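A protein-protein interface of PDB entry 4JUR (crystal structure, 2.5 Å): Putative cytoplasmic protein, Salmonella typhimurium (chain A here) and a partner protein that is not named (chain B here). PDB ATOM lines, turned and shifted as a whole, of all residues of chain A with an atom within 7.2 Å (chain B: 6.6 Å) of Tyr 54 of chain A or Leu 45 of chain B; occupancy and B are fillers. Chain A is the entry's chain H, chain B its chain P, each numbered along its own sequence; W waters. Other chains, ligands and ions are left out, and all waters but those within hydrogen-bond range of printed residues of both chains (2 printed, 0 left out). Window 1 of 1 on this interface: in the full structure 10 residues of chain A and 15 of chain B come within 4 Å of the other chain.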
ATOM      1  N   LYS A  48      30.972  -9.198  12.921  1.00  0.00           N
ATOM      2  CA  LYS A  48      31.440  -9.422  11.556  1.00  0.00           C
ATOM      3  C   LYS A  48      30.256  -9.677  10.616  1.00  0.00           C
ATOM      4  O   LYS A  48      30.134  -9.071   9.542  1.00  0.00           O
ATOM      5  CB  LYS A  48      32.448 -10.569  11.492  1.00  0.00           C
ATOM      6  CG  LYS A  48      32.774 -10.983  10.067  1.00  0.00           C
ATOM      7  CD  LYS A  48      34.124 -11.692   9.951  1.00  0.00           C
ATOM      8  CE  LYS A  48      35.310 -10.735  10.221  1.00  0.00           C
ATOM      9  NZ  LYS A  48      35.313  -9.498   9.361  1.00  0.00           N
ATOM     10  N   ASN A  49      29.370 -10.563  11.047  1.00  0.00           N
ATOM     11  CA  ASN A  49      28.163 -10.836  10.284  1.00  0.00           C
ATOM     12  C   ASN A  49      27.212  -9.644  10.181  1.00  0.00           C
ATOM     13  O   ASN A  49      26.564  -9.448   9.160  1.00  0.00           O
ATOM     14  CB  ASN A  49      27.450 -12.063  10.838  1.00  0.00           C
ATOM     15  CG  ASN A  49      28.186 -13.338  10.515  1.00  0.00           C
ATOM     16  OD1 ASN A  49      28.367 -13.667   9.342  1.00  0.00           O
ATOM     17  ND2 ASN A  49      28.617 -14.063  11.543  1.00  0.00           N
ATOM     18  N   ILE A  50      27.138  -8.840  11.231  1.00  0.00           N
ATOM     19  CA  ILE A  50      26.302  -7.659  11.163  1.00  0.00           C
ATOM     20  C   ILE A  50      26.885  -6.618  10.214  1.00  0.00           C
ATOM     21  O   ILE A  50      26.164  -6.041   9.395  1.00  0.00           O
ATOM     22  CB  ILE A  50      26.046  -7.067  12.549  1.00  0.00           C
ATOM     23  CG1 ILE A  50      25.124  -8.010  13.311  1.00  0.00           C
ATOM     24  CG2 ILE A  50      25.410  -5.683  12.423  1.00  0.00           C
ATOM     25  CD1 ILE A  50      24.815  -7.579  14.705  1.00  0.00           C
ATOM     26  N   THR A  51      28.191  -6.393  10.326  1.00  0.00           N
ATOM     27  CA  THR A  51      28.904  -5.479   9.438  1.00  0.00           C
ATOM     28  C   THR A  51      28.705  -5.924   7.983  1.00  0.00           C
ATOM     29  O   THR A  51      28.566  -5.095   7.071  1.00  0.00           O
ATOM     30  CB  THR A  51      30.432  -5.449   9.750  1.00  0.00           C
ATOM     31  OG1 THR A  51      30.664  -4.938  11.075  1.00  0.00           O
ATOM     32  CG2 THR A  51      31.167  -4.587   8.738  1.00  0.00           C
ATOM     33  N   GLY A  52      28.680  -7.241   7.780  1.00  0.00           N
ATOM     34  CA  GLY A  52      28.484  -7.801   6.459  1.00  0.00           C
ATOM     35  C   GLY A  52      27.069  -7.660   5.927  1.00  0.00           C
ATOM     36  O   GLY A  52      26.852  -7.775   4.724  1.00  0.00           O
ATOM     37  N   GLY A  53      26.104  -7.415   6.808  1.00  0.00           N
ATOM     38  CA  GLY A  53      24.722  -7.295   6.383  1.00  0.00           C
ATOM     39  C   GLY A  53      24.036  -8.651   6.245  1.00  0.00           C
ATOM     40  O   GLY A  53      22.912  -8.748   5.718  1.00  0.00           O
ATOM     41  N   TYR A  54      24.719  -9.701   6.707  1.00  0.00           N
ATOM     42  CA  TYR A  54      24.169 -11.046   6.678  1.00  0.00           C
ATOM     43  C   TYR A  54      23.049 -11.137   7.698  1.00  0.00           C
ATOM     44  O   TYR A  54      21.994 -11.656   7.395  1.00  0.00           O
ATOM     45  CB  TYR A  54      25.246 -12.100   6.962  1.00  0.00           C
ATOM     46  CG  TYR A  54      26.474 -12.003   6.070  1.00  0.00           C
ATOM     47  CD1 TYR A  54      26.496 -12.579   4.812  1.00  0.00           C
ATOM     48  CD2 TYR A  54      27.622 -11.348   6.495  1.00  0.00           C
ATOM     49  CE1 TYR A  54      27.631 -12.493   3.988  1.00  0.00           C
ATOM     50  CE2 TYR A  54      28.762 -11.263   5.681  1.00  0.00           C
ATOM     51  CZ  TYR A  54      28.753 -11.841   4.433  1.00  0.00           C
ATOM     52  OH  TYR A  54      29.859 -11.759   3.633  1.00  0.00           O
ATOM     53  N   PHE A  55      23.282 -10.604   8.900  1.00  0.00           N
ATOM     54  CA  PHE A  55      22.260 -10.558   9.951  1.00  0.00           C
ATOM     55  C   PHE A  55      21.565  -9.213   9.902  1.00  0.00           C
ATOM     56  O   PHE A  55      22.218  -8.171   9.950  1.00  0.00           O
ATOM     57  CB  PHE A  55      22.870 -10.693  11.343  1.00  0.00           C
ATOM     58  CG  PHE A  55      23.634 -11.966  11.568  1.00  0.00           C
ATOM     59  CD1 PHE A  55      23.536 -13.036  10.678  1.00  0.00           C
ATOM     60  CD2 PHE A  55      24.446 -12.098  12.689  1.00  0.00           C
ATOM     61  CE1 PHE A  55      24.252 -14.216  10.901  1.00  0.00           C
ATOM     62  CE2 PHE A  55      25.153 -13.269  12.926  1.00  0.00           C
ATOM     63  CZ  PHE A  55      25.057 -14.334  12.028  1.00  0.00           C
ATOM     64  N   GLN A  56      20.241  -9.224   9.822  1.00  0.00           N
ATOM     65  CA  GLN A  56      19.490  -7.974   9.796  1.00  0.00           C
ATOM     66  C   GLN A  56      18.524  -7.926  10.963  1.00  0.00           C
ATOM     67  O   GLN A  56      18.101  -6.860  11.362  1.00  0.00           O
ATOM     68  CB  GLN A  56      18.741  -7.816   8.468  1.00  0.00           C
ATOM     69  CG  GLN A  56      19.667  -7.808   7.253  1.00  0.00           C
ATOM     70  CD  GLN A  56      20.051  -6.410   6.794  1.00  0.00           C
ATOM     71  OE1 GLN A  56      19.185  -5.567   6.579  1.00  0.00           O
ATOM     72  NE2 GLN A  56      21.346  -6.168   6.625  1.00  0.00           N
ATOM     73  N   ASN A  57      18.176  -9.086  11.510  1.00  0.00           N
ATOM     74  CA  ASN A  57      17.217  -9.140  12.605  1.00  0.00           C
ATOM     75  C   ASN A  57      17.928  -9.359  13.926  1.00  0.00           C
ATOM     76  O   ASN A  57      18.450 -10.433  14.165  1.00  0.00           O
ATOM     77  CB  ASN A  57      16.211 -10.267  12.372  1.00  0.00           C
ATOM     78  CG  ASN A  57      15.071 -10.253  13.378  1.00  0.00           C
ATOM     79  OD1 ASN A  57      15.047  -9.429  14.295  1.00  0.00           O
ATOM     80  ND2 ASN A  57      14.108 -11.143  13.192  1.00  0.00           N
ATOM     81  N   TYR A  93      21.325 -16.573  15.857  1.00  0.00           N
ATOM     82  CA  TYR A  93      20.951 -15.531  14.904  1.00  0.00           C
ATOM     83  C   TYR A  93      19.654 -15.785  14.155  1.00  0.00           C
ATOM     84  O   TYR A  93      19.264 -14.983  13.300  1.00  0.00           O
ATOM     85  CB  TYR A  93      22.081 -15.256  13.917  1.00  0.00           C
ATOM     86  CG  TYR A  93      22.690 -16.493  13.287  1.00  0.00           C
ATOM     87  CD1 TYR A  93      22.464 -16.803  11.946  1.00  0.00           C
ATOM     88  CD2 TYR A  93      23.501 -17.345  14.027  1.00  0.00           C
ATOM     89  CE1 TYR A  93      23.033 -17.923  11.368  1.00  0.00           C
ATOM     90  CE2 TYR A  93      24.064 -18.457  13.462  1.00  0.00           C
ATOM     91  CZ  TYR A  93      23.833 -18.745  12.134  1.00  0.00           C
ATOM     92  OH  TYR A  93      24.412 -19.866  11.583  1.00  0.00           O
ATOM     93  N   ARG A  94      18.985 -16.887  14.487  1.00  0.00           N
ATOM     94  CA  ARG A  94      17.714 -17.203  13.866  1.00  0.00           C
ATOM     95  C   ARG A  94      16.585 -17.177  14.875  1.00  0.00           C
ATOM     96  O   ARG A  94      16.660 -17.829  15.905  1.00  0.00           O
ATOM     97  CB  ARG A  94      17.773 -18.558  13.165  1.00  0.00           C
ATOM     98  CG  ARG A  94      18.694 -18.575  11.985  1.00  0.00           C
ATOM     99  CD  ARG A  94      18.595 -19.884  11.192  1.00  0.00           C
ATOM    100  NE  ARG A  94      19.157 -19.663   9.861  1.00  0.00           N
ATOM    101  CZ  ARG A  94      20.270 -20.211   9.397  1.00  0.00           C
ATOM    102  NH1 ARG A  94      20.944 -21.083  10.129  1.00  0.00           N
ATOM    103  NH2 ARG A  94      20.690 -19.894   8.180  1.00  0.00           N
ATOM    104  N   ILE B  14      16.389 -21.922  -1.566  1.00  0.00           N
ATOM    105  CA  ILE B  14      16.533 -20.908  -0.544  1.00  0.00           C
ATOM    106  C   ILE B  14      17.961 -20.324  -0.598  1.00  0.00           C
ATOM    107  O   ILE B  14      18.138 -19.087  -0.614  1.00  0.00           O
ATOM    108  CB  ILE B  14      16.168 -21.496   0.853  1.00  0.00           C
ATOM    109  CG1 ILE B  14      14.665 -21.715   0.962  1.00  0.00           C
ATOM    110  CG2 ILE B  14      16.651 -20.609   1.992  1.00  0.00           C
ATOM    111  CD1 ILE B  14      14.266 -22.594   2.120  1.00  0.00           C
ATOM    112  N   TRP B  18      19.090 -16.550  -1.868  1.00  0.00           N
ATOM    113  CA  TRP B  18      19.887 -15.669  -1.030  1.00  0.00           C
ATOM    114  C   TRP B  18      20.998 -15.062  -1.881  1.00  0.00           C
ATOM    115  O   TRP B  18      21.266 -13.857  -1.790  1.00  0.00           O
ATOM    116  CB  TRP B  18      20.503 -16.412   0.150  1.00  0.00           C
ATOM    117  CG  TRP B  18      21.358 -15.529   0.987  1.00  0.00           C
ATOM    118  CD1 TRP B  18      20.962 -14.777   2.056  1.00  0.00           C
ATOM    119  CD2 TRP B  18      22.760 -15.291   0.833  1.00  0.00           C
ATOM    120  NE1 TRP B  18      22.025 -14.092   2.578  1.00  0.00           N
ATOM    121  CE2 TRP B  18      23.144 -14.387   1.849  1.00  0.00           C
ATOM    122  CE3 TRP B  18      23.728 -15.748  -0.065  1.00  0.00           C
ATOM    123  CZ2 TRP B  18      24.449 -13.935   1.991  1.00  0.00           C
ATOM    124  CZ3 TRP B  18      25.029 -15.291   0.078  1.00  0.00           C
ATOM    125  CH2 TRP B  18      25.375 -14.392   1.101  1.00  0.00           C
ATOM    126  N   ARG B  22      21.256 -11.102  -2.849  1.00  0.00           N
ATOM    127  CA  ARG B  22      22.430 -10.388  -2.413  1.00  0.00           C
ATOM    128  C   ARG B  22      23.136  -9.760  -3.586  1.00  0.00           C
ATOM    129  O   ARG B  22      23.544  -8.603  -3.530  1.00  0.00           O
ATOM    130  CB  ARG B  22      23.406 -11.281  -1.656  1.00  0.00           C
ATOM    131  CG  ARG B  22      24.435 -10.416  -0.971  1.00  0.00           C
ATOM    132  CD  ARG B  22      25.177 -11.135   0.072  1.00  0.00           C
ATOM    133  NE  ARG B  22      26.052 -10.227   0.789  1.00  0.00           N
ATOM    134  CZ  ARG B  22      25.641  -9.439   1.776  1.00  0.00           C
ATOM    135  NH1 ARG B  22      24.365  -9.435   2.144  1.00  0.00           N
ATOM    136  NH2 ARG B  22      26.508  -8.644   2.386  1.00  0.00           N
ATOM    137  N   LYS B  26      24.410  -6.022  -4.599  1.00  0.00           N
ATOM    138  CA  LYS B  26      25.748  -5.546  -4.965  1.00  0.00           C
ATOM    139  C   LYS B  26      25.737  -4.759  -6.263  1.00  0.00           C
ATOM    140  O   LYS B  26      26.602  -3.918  -6.467  1.00  0.00           O
ATOM    141  CB  LYS B  26      26.760  -6.689  -5.093  1.00  0.00           C
ATOM    142  CG  LYS B  26      26.946  -7.505  -3.827  1.00  0.00           C
ATOM    143  CD  LYS B  26      28.270  -8.252  -3.813  1.00  0.00           C
ATOM    144  CE  LYS B  26      28.508  -8.829  -2.426  1.00  0.00           C
ATOM    145  NZ  LYS B  26      28.101  -7.851  -1.352  1.00  0.00           N
ATOM    146  N   ASP B  38      19.033  -6.415   0.758  1.00  0.00           N
ATOM    147  CA  ASP B  38      19.632  -6.996   1.956  1.00  0.00           C
ATOM    148  C   ASP B  38      18.607  -7.548   2.936  1.00  0.00           C
ATOM    149  O   ASP B  38      18.850  -8.572   3.590  1.00  0.00           O
ATOM    150  CB  ASP B  38      20.576  -6.008   2.642  1.00  0.00           C
ATOM    151  CG  ASP B  38      21.914  -5.887   1.914  1.00  0.00           C
ATOM    152  OD1 ASP B  38      22.023  -6.399   0.773  1.00  0.00           O
ATOM    153  OD2 ASP B  38      22.856  -5.282   2.473  1.00  0.00           O
ATOM    154  N   SER B  40      15.647  -8.702   1.960  1.00  0.00           N
ATOM    155  CA  SER B  40      15.222  -9.902   1.231  1.00  0.00           C
ATOM    156  C   SER B  40      16.153 -11.100   1.463  1.00  0.00           C
ATOM    157  O   SER B  40      15.729 -12.198   1.907  1.00  0.00           O
ATOM    158  CB  SER B  40      15.140  -9.579  -0.266  1.00  0.00           C
ATOM    159  OG  SER B  40      14.181  -8.557  -0.527  1.00  0.00           O
ATOM    160  N   ALA B  41      17.428 -10.885   1.170  1.00  0.00           N
ATOM    161  CA  ALA B  41      18.451 -11.887   1.426  1.00  0.00           C
ATOM    162  C   ALA B  41      18.392 -12.390   2.869  1.00  0.00           C
ATOM    163  O   ALA B  41      18.498 -13.597   3.106  1.00  0.00           O
ATOM    164  CB  ALA B  41      19.815 -11.340   1.122  1.00  0.00           C
ATOM    165  N   ALA B  42      18.220 -11.475   3.825  1.00  0.00           N
ATOM    166  CA  ALA B  42      18.068 -11.867   5.226  1.00  0.00           C
ATOM    167  C   ALA B  42      16.909 -12.865   5.428  1.00  0.00           C
ATOM    168  O   ALA B  42      17.034 -13.856   6.184  1.00  0.00           O
ATOM    169  CB  ALA B  42      17.865 -10.634   6.105  1.00  0.00           C
ATOM    170  N   ALA B  43      15.791 -12.600   4.756  1.00  0.00           N
ATOM    171  CA  ALA B  43      14.664 -13.521   4.819  1.00  0.00           C
ATOM    172  C   ALA B  43      15.037 -14.922   4.320  1.00  0.00           C
ATOM    173  O   ALA B  43      14.627 -15.922   4.911  1.00  0.00           O
ATOM    174  CB  ALA B  43      13.461 -12.976   4.061  1.00  0.00           C
ATOM    175  N   TRP B  44      15.817 -15.012   3.246  1.00  0.00           N
ATOM    176  CA  TRP B  44      16.252 -16.348   2.829  1.00  0.00           C
ATOM    177  C   TRP B  44      17.225 -16.962   3.832  1.00  0.00           C
ATOM    178  O   TRP B  44      17.206 -18.173   4.043  1.00  0.00           O
ATOM    179  CB  TRP B  44      16.849 -16.378   1.407  1.00  0.00           C
ATOM    180  CG  TRP B  44      15.906 -15.919   0.349  1.00  0.00           C
ATOM    181  CD1 TRP B  44      15.902 -14.707  -0.262  1.00  0.00           C
ATOM    182  CD2 TRP B  44      14.805 -16.651  -0.210  1.00  0.00           C
ATOM    183  NE1 TRP B  44      14.885 -14.634  -1.186  1.00  0.00           N
ATOM    184  CE2 TRP B  44      14.194 -15.815  -1.176  1.00  0.00           C
ATOM    185  CE3 TRP B  44      14.299 -17.940  -0.021  1.00  0.00           C
ATOM    186  CZ2 TRP B  44      13.088 -16.226  -1.940  1.00  0.00           C
ATOM    187  CZ3 TRP B  44      13.198 -18.343  -0.777  1.00  0.00           C
ATOM    188  CH2 TRP B  44      12.607 -17.487  -1.723  1.00  0.00           C
ATOM    189  N   LEU B  45      18.070 -16.153   4.470  1.00  0.00           N
ATOM    190  CA  LEU B  45      19.025 -16.724   5.450  1.00  0.00           C
ATOM    191  C   LEU B  45      18.340 -17.318   6.710  1.00  0.00           C
ATOM    192  O   LEU B  45      18.783 -18.337   7.246  1.00  0.00           O
ATOM    193  CB  LEU B  45      20.125 -15.727   5.801  1.00  0.00           C
ATOM    194  CG  LEU B  45      21.251 -16.103   6.760  1.00  0.00           C
ATOM    195  CD1 LEU B  45      22.474 -15.236   6.470  1.00  0.00           C
ATOM    196  CD2 LEU B  45      20.834 -15.918   8.212  1.00  0.00           C
ATOM    197  N   GLU B  46      17.263 -16.688   7.168  1.00  0.00           N
ATOM    198  CA  GLU B  46      16.493 -17.217   8.296  1.00  0.00           C
ATOM    199  C   GLU B  46      15.927 -18.642   8.053  1.00  0.00           C
ATOM    200  O   GLU B  46      15.920 -19.485   8.953  1.00  0.00           O
ATOM    201  CB  GLU B  46      15.361 -16.244   8.651  1.00  0.00           C
ATOM    202  CG  GLU B  46      14.251 -16.858   9.501  1.00  0.00           C
ATOM    203  CD  GLU B  46      14.580 -16.898  11.014  1.00  0.00           C
ATOM    204  OE1 GLU B  46      15.449 -16.112  11.476  1.00  0.00           O
ATOM    205  OE2 GLU B  46      13.957 -17.710  11.737  1.00  0.00           O
ATOM    206  N   ALA B  47      15.467 -18.901   6.831  1.00  0.00           N
ATOM    207  CA  ALA B  47      14.844 -20.176   6.476  1.00  0.00           C
ATOM    208  C   ALA B  47      15.849 -21.249   6.106  1.00  0.00           C
ATOM    209  O   ALA B  47      15.524 -22.436   6.119  1.00  0.00           O
ATOM    210  CB  ALA B  47      13.870 -19.990   5.321  1.00  0.00           C
ATOM    211  N   SER B  48      17.060 -20.835   5.750  1.00  0.00           N
ATOM    212  CA  SER B  48      18.100 -21.780   5.395  1.00  0.00           C
ATOM    213  C   SER B  48      18.571 -22.547   6.596  1.00  0.00           C
ATOM    214  O   SER B  48      18.586 -22.030   7.712  1.00  0.00           O
ATOM    215  CB  SER B  48      19.308 -21.067   4.813  1.00  0.00           C
ATOM    216  OG  SER B  48      20.391 -21.980   4.755  1.00  0.00           O
ATOM    217  N   ASN B  49      19.008 -23.773   6.361  1.00  0.00           N
ATOM    218  CA  ASN B  49      19.501 -24.597   7.447  1.00  0.00           C
ATOM    219  C   ASN B  49      21.025 -24.601   7.514  1.00  0.00           C
ATOM    220  O   ASN B  49      21.609 -25.294   8.335  1.00  0.00           O
ATOM    221  CB  ASN B  49      18.908 -26.028   7.393  1.00  0.00           C
ATOM    222  CG  ASN B  49      19.328 -26.820   6.143  1.00  0.00           C
ATOM    223  OD1 ASN B  49      20.270 -26.451   5.430  1.00  0.00           O
ATOM    224  ND2 ASN B  49      18.625 -27.932   5.886  1.00  0.00           N
ATOM    225  N   LEU B  50      21.664 -23.812   6.659  1.00  0.00           N
ATOM    226  CA  LEU B  50      23.113 -23.820   6.586  1.00  0.00           C
ATOM    227  C   LEU B  50      23.693 -22.900   7.629  1.00  0.00           C
ATOM    228  O   LEU B  50      23.025 -21.966   8.070  1.00  0.00           O
ATOM    229  CB  LEU B  50      23.569 -23.334   5.212  1.00  0.00           C
ATOM    230  CG  LEU B  50      23.226 -24.205   4.008  1.00  0.00           C
ATOM    231  CD1 LEU B  50      23.723 -23.586   2.699  1.00  0.00           C
ATOM    232  CD2 LEU B  50      23.799 -25.590   4.202  1.00  0.00           C
ATOM    233  N   ALA B  52      26.123 -19.855   9.009  1.00  0.00           N
ATOM    234  CA  ALA B  52      26.477 -18.509   8.574  1.00  0.00           C
ATOM    235  C   ALA B  52      27.715 -18.454   7.677  1.00  0.00           C
ATOM    236  O   ALA B  52      27.778 -17.675   6.702  1.00  0.00           O
ATOM    237  CB  ALA B  52      26.702 -17.658   9.793  1.00  0.00           C
ATOM    238  N   PHE B  55      27.339 -18.569   3.986  1.00  0.00           N
ATOM    239  CA  PHE B  55      26.905 -17.330   3.388  1.00  0.00           C
ATOM    240  C   PHE B  55      28.072 -16.379   3.231  1.00  0.00           C
ATOM    241  O   PHE B  55      28.154 -15.673   2.231  1.00  0.00           O
ATOM    242  CB  PHE B  55      25.761 -16.708   4.175  1.00  0.00           C
ATOM    243  CG  PHE B  55      24.540 -17.565   4.217  1.00  0.00           C
ATOM    244  CD1 PHE B  55      23.506 -17.361   3.325  1.00  0.00           C
ATOM    245  CD2 PHE B  55      24.426 -18.585   5.153  1.00  0.00           C
ATOM    246  CE1 PHE B  55      22.389 -18.158   3.372  1.00  0.00           C
ATOM    247  CE2 PHE B  55      23.312 -19.384   5.202  1.00  0.00           C
ATOM    248  CZ  PHE B  55      22.299 -19.188   4.318  1.00  0.00           C
ATOM    249  N   GLU B  56      28.993 -16.393   4.191  1.00  0.00           N
ATOM    250  CA  GLU B  56      30.226 -15.587   4.037  1.00  0.00           C
ATOM    251  C   GLU B  56      31.100 -15.974   2.819  1.00  0.00           C
ATOM    252  O   GLU B  56      31.525 -15.105   2.010  1.00  0.00           O
ATOM    253  CB  GLU B  56      31.064 -15.653   5.315  1.00  0.00           C
ATOM    254  CG  GLU B  56      32.386 -14.895   5.241  1.00  0.00           C
ATOM    255  CD  GLU B  56      33.061 -14.820   6.606  1.00  0.00           C
ATOM    256  OE1 GLU B  56      32.476 -15.379   7.579  1.00  0.00           O
ATOM    257  OE2 GLU B  56      34.153 -14.197   6.705  1.00  0.00           O
ATOM    258  N   LYS B  57      31.374 -17.274   2.700  1.00  0.00           N
ATOM    259  CA  LYS B  57      32.101 -17.803   1.537  1.00  0.00           C
ATOM    260  C   LYS B  57      31.385 -17.518   0.199  1.00  0.00           C
ATOM    261  O   LYS B  57      32.025 -17.173  -0.826  1.00  0.00           O
ATOM    262  CB  LYS B  57      32.323 -19.300   1.697  1.00  0.00           C
ATOM    263  CG  LYS B  57      33.003 -19.698   3.008  1.00  0.00           C
ATOM    264  CD  LYS B  57      34.532 -19.662   2.919  1.00  0.00           C
ATOM    265  N   ALA B  58      30.058 -17.652   0.215  1.00  0.00           N
ATOM    266  CA  ALA B  58      29.253 -17.379  -0.966  1.00  0.00           C
ATOM    267  C   ALA B  58      29.316 -15.907  -1.345  1.00  0.00           C
ATOM    268  O   ALA B  58      29.334 -15.573  -2.529  1.00  0.00           O
ATOM    269  CB  ALA B  58      27.828 -17.837  -0.775  1.00  0.00           C
ATOM    270  N   ASP B  59      29.359 -15.021  -0.355  1.00  0.00           N
ATOM    271  CA  ASP B  59      29.530 -13.611  -0.661  1.00  0.00           C
ATOM    272  C   ASP B  59      30.858 -13.413  -1.377  1.00  0.00           C
ATOM    273  O   ASP B  59      30.904 -12.745  -2.426  1.00  0.00           O
ATOM    274  CB  ASP B  59      29.468 -12.740   0.582  1.00  0.00           C
ATOM    275  CG  ASP B  59      29.499 -11.253   0.247  1.00  0.00           C
ATOM    276  OD1 ASP B  59      28.403 -10.645   0.106  1.00  0.00           O
ATOM    277  OD2 ASP B  59      30.618 -10.697   0.117  1.00  0.00           O
ATOM    278  N   GLU B  60      31.926 -14.010  -0.837  1.00  0.00           N
ATOM    279  CA  GLU B  60      33.212 -13.993  -1.557  1.00  0.00           C
ATOM    280  C   GLU B  60      33.087 -14.415  -3.044  1.00  0.00           C
ATOM    281  O   GLU B  60      33.519 -13.680  -3.960  1.00  0.00           O
ATOM    282  CB  GLU B  60      34.260 -14.851  -0.846  1.00  0.00           C
ATOM    283  CG  GLU B  60      34.680 -14.324   0.534  1.00  0.00           C
HETATM  284  O   HOH W   1      21.419 -12.447   4.724  1.00  0.00           O
HETATM  285  O   HOH W   2      14.936 -13.220  10.866  1.00  0.00           O
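Of the 23 printed residues of chain B, 12 touch a printed residue of chain A. Printed residues of chain B that touch a printed residue of chain A: Trp 18, Arg 22, Asp 38, Ala 42, Leu 45, Glu 46, Ser 48, Leu 50, Ala 52, Phe 55, Glu 56 and Asp 59. Of the 12 printed residues of chain A, 6 touch a printed residue of chain B. Printed residues of chain A that touch a printed residue of chain B: Gly 52, Gly 53, Tyr 54, Gln 56, Tyr 93 and Arg 94. Hydrophobic or aromatic side chains of chain A within 4 Å of the printed part of chain B: Tyr 54 and Tyr 93. Among the printed residues, 14 pairs touch across the chains.
Gly 53 of chain A touches Arg 22 of chain B. Trp 18 of chain B touches Tyr 54 of chain A. CD1 of Leu 45 of chain B touches O of Tyr 54 of chain A, 3.7 Å away. CE1 of Tyr 54 of chain A touches O of Phe 55 of chain B (3.7 Å). Glu 56 of chain B touches Tyr 54 of chain A. Tyr 54 of chain A touches Asp 59 of chain B (OH to CB, 3.2 Å). Gln 56 of chain A touches Asp 38 of chain B (CG to O, 3.8 Å). Gln 56 of chain A touches Ala 42 of chain B.
The backbone carbonyl oxygen (O) of Asn 49 of chain A lies within hydrogen-bond range of the backbone NH (N) of Tyr 54 of chain A. The backbone NH (N) of Leu 50 of chain B sits at hydrogen-bond distance from the side-chain hydroxyl (OG) of Ser 48 of chain B (2.9 Å). NE2 of Gln 56 of chain A sits at hydrogen-bond distance from O of Gly 53 of chain A. The side-chain amino group (NZ) of Lys 26 of chain B is in salt-bridge range of the side-chain carboxylate (OD1) of Asp 59 of chain B, at 3.2 Å. NE of Arg 22 of chain B lies within salt-bridge range of OD1 of Asp 59 of chain B (2.5 Å).
Of the printed residues of chain B, Gln 56 of chain A touches Asp 38 (3.8 Å) and Ala 42 (3.5 Å). Of the printed residues of chain A, Trp 18 of chain B touches Tyr 54. Ala 43 of chain B touches none of the printed residues of chain A. Leu 45 of chain B touches just these residues of chain A: Tyr 54 (3.7 Å) and Arg 94 (2.6 Å). Printed residues of chain A within 4 Å of Ser 48 of chain B: Arg 94 (3.0 Å). Printed residues of chain A within 4 Å of Leu 50 of chain B: Arg 94. Glu 60 of chain B touches none of the printed residues of chain A. The nearest residue of chain B that does not touch Tyr 54 of chain A is Arg 22 of chain B (4.2 Å).
Water W1 lies within hydrogen-bond range of NE1 of Trp 18 of chain B, O of Tyr 54 of chain A and N of Ala 42 of chain B. Water W2 lies within hydrogen-bond range of OE1 of Glu 46 of chain B and ND2 of Asn 57 of chain A.
The guanidinium group of Arg 94 of chain A lies within hydrogen-bond range of the backbone carbonyl oxygen of Leu 45 of chain B (2.6 Å). NH2 of Arg 94 of chain A sits close to O of Ser 48 of chain B. O of Leu 50 of chain B lies within hydrogen-bond range of NH1 of Arg 94 of chain A. O of Glu 46 of chain B sits at hydrogen-bond distance from NE of Arg 94 of chain A (3.4 Å). The backbone carbonyl oxygen (O) of Gly 52 of chain A lies within hydrogen-bond range of the guanidinium group (NH2) of Arg 22 of chain B (2.5 Å). The side-chain hydroxyl (OH) of Tyr 93 of chain A sits at hydrogen-bond distance from the backbone NH (N) of Ala 52 of chain B.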
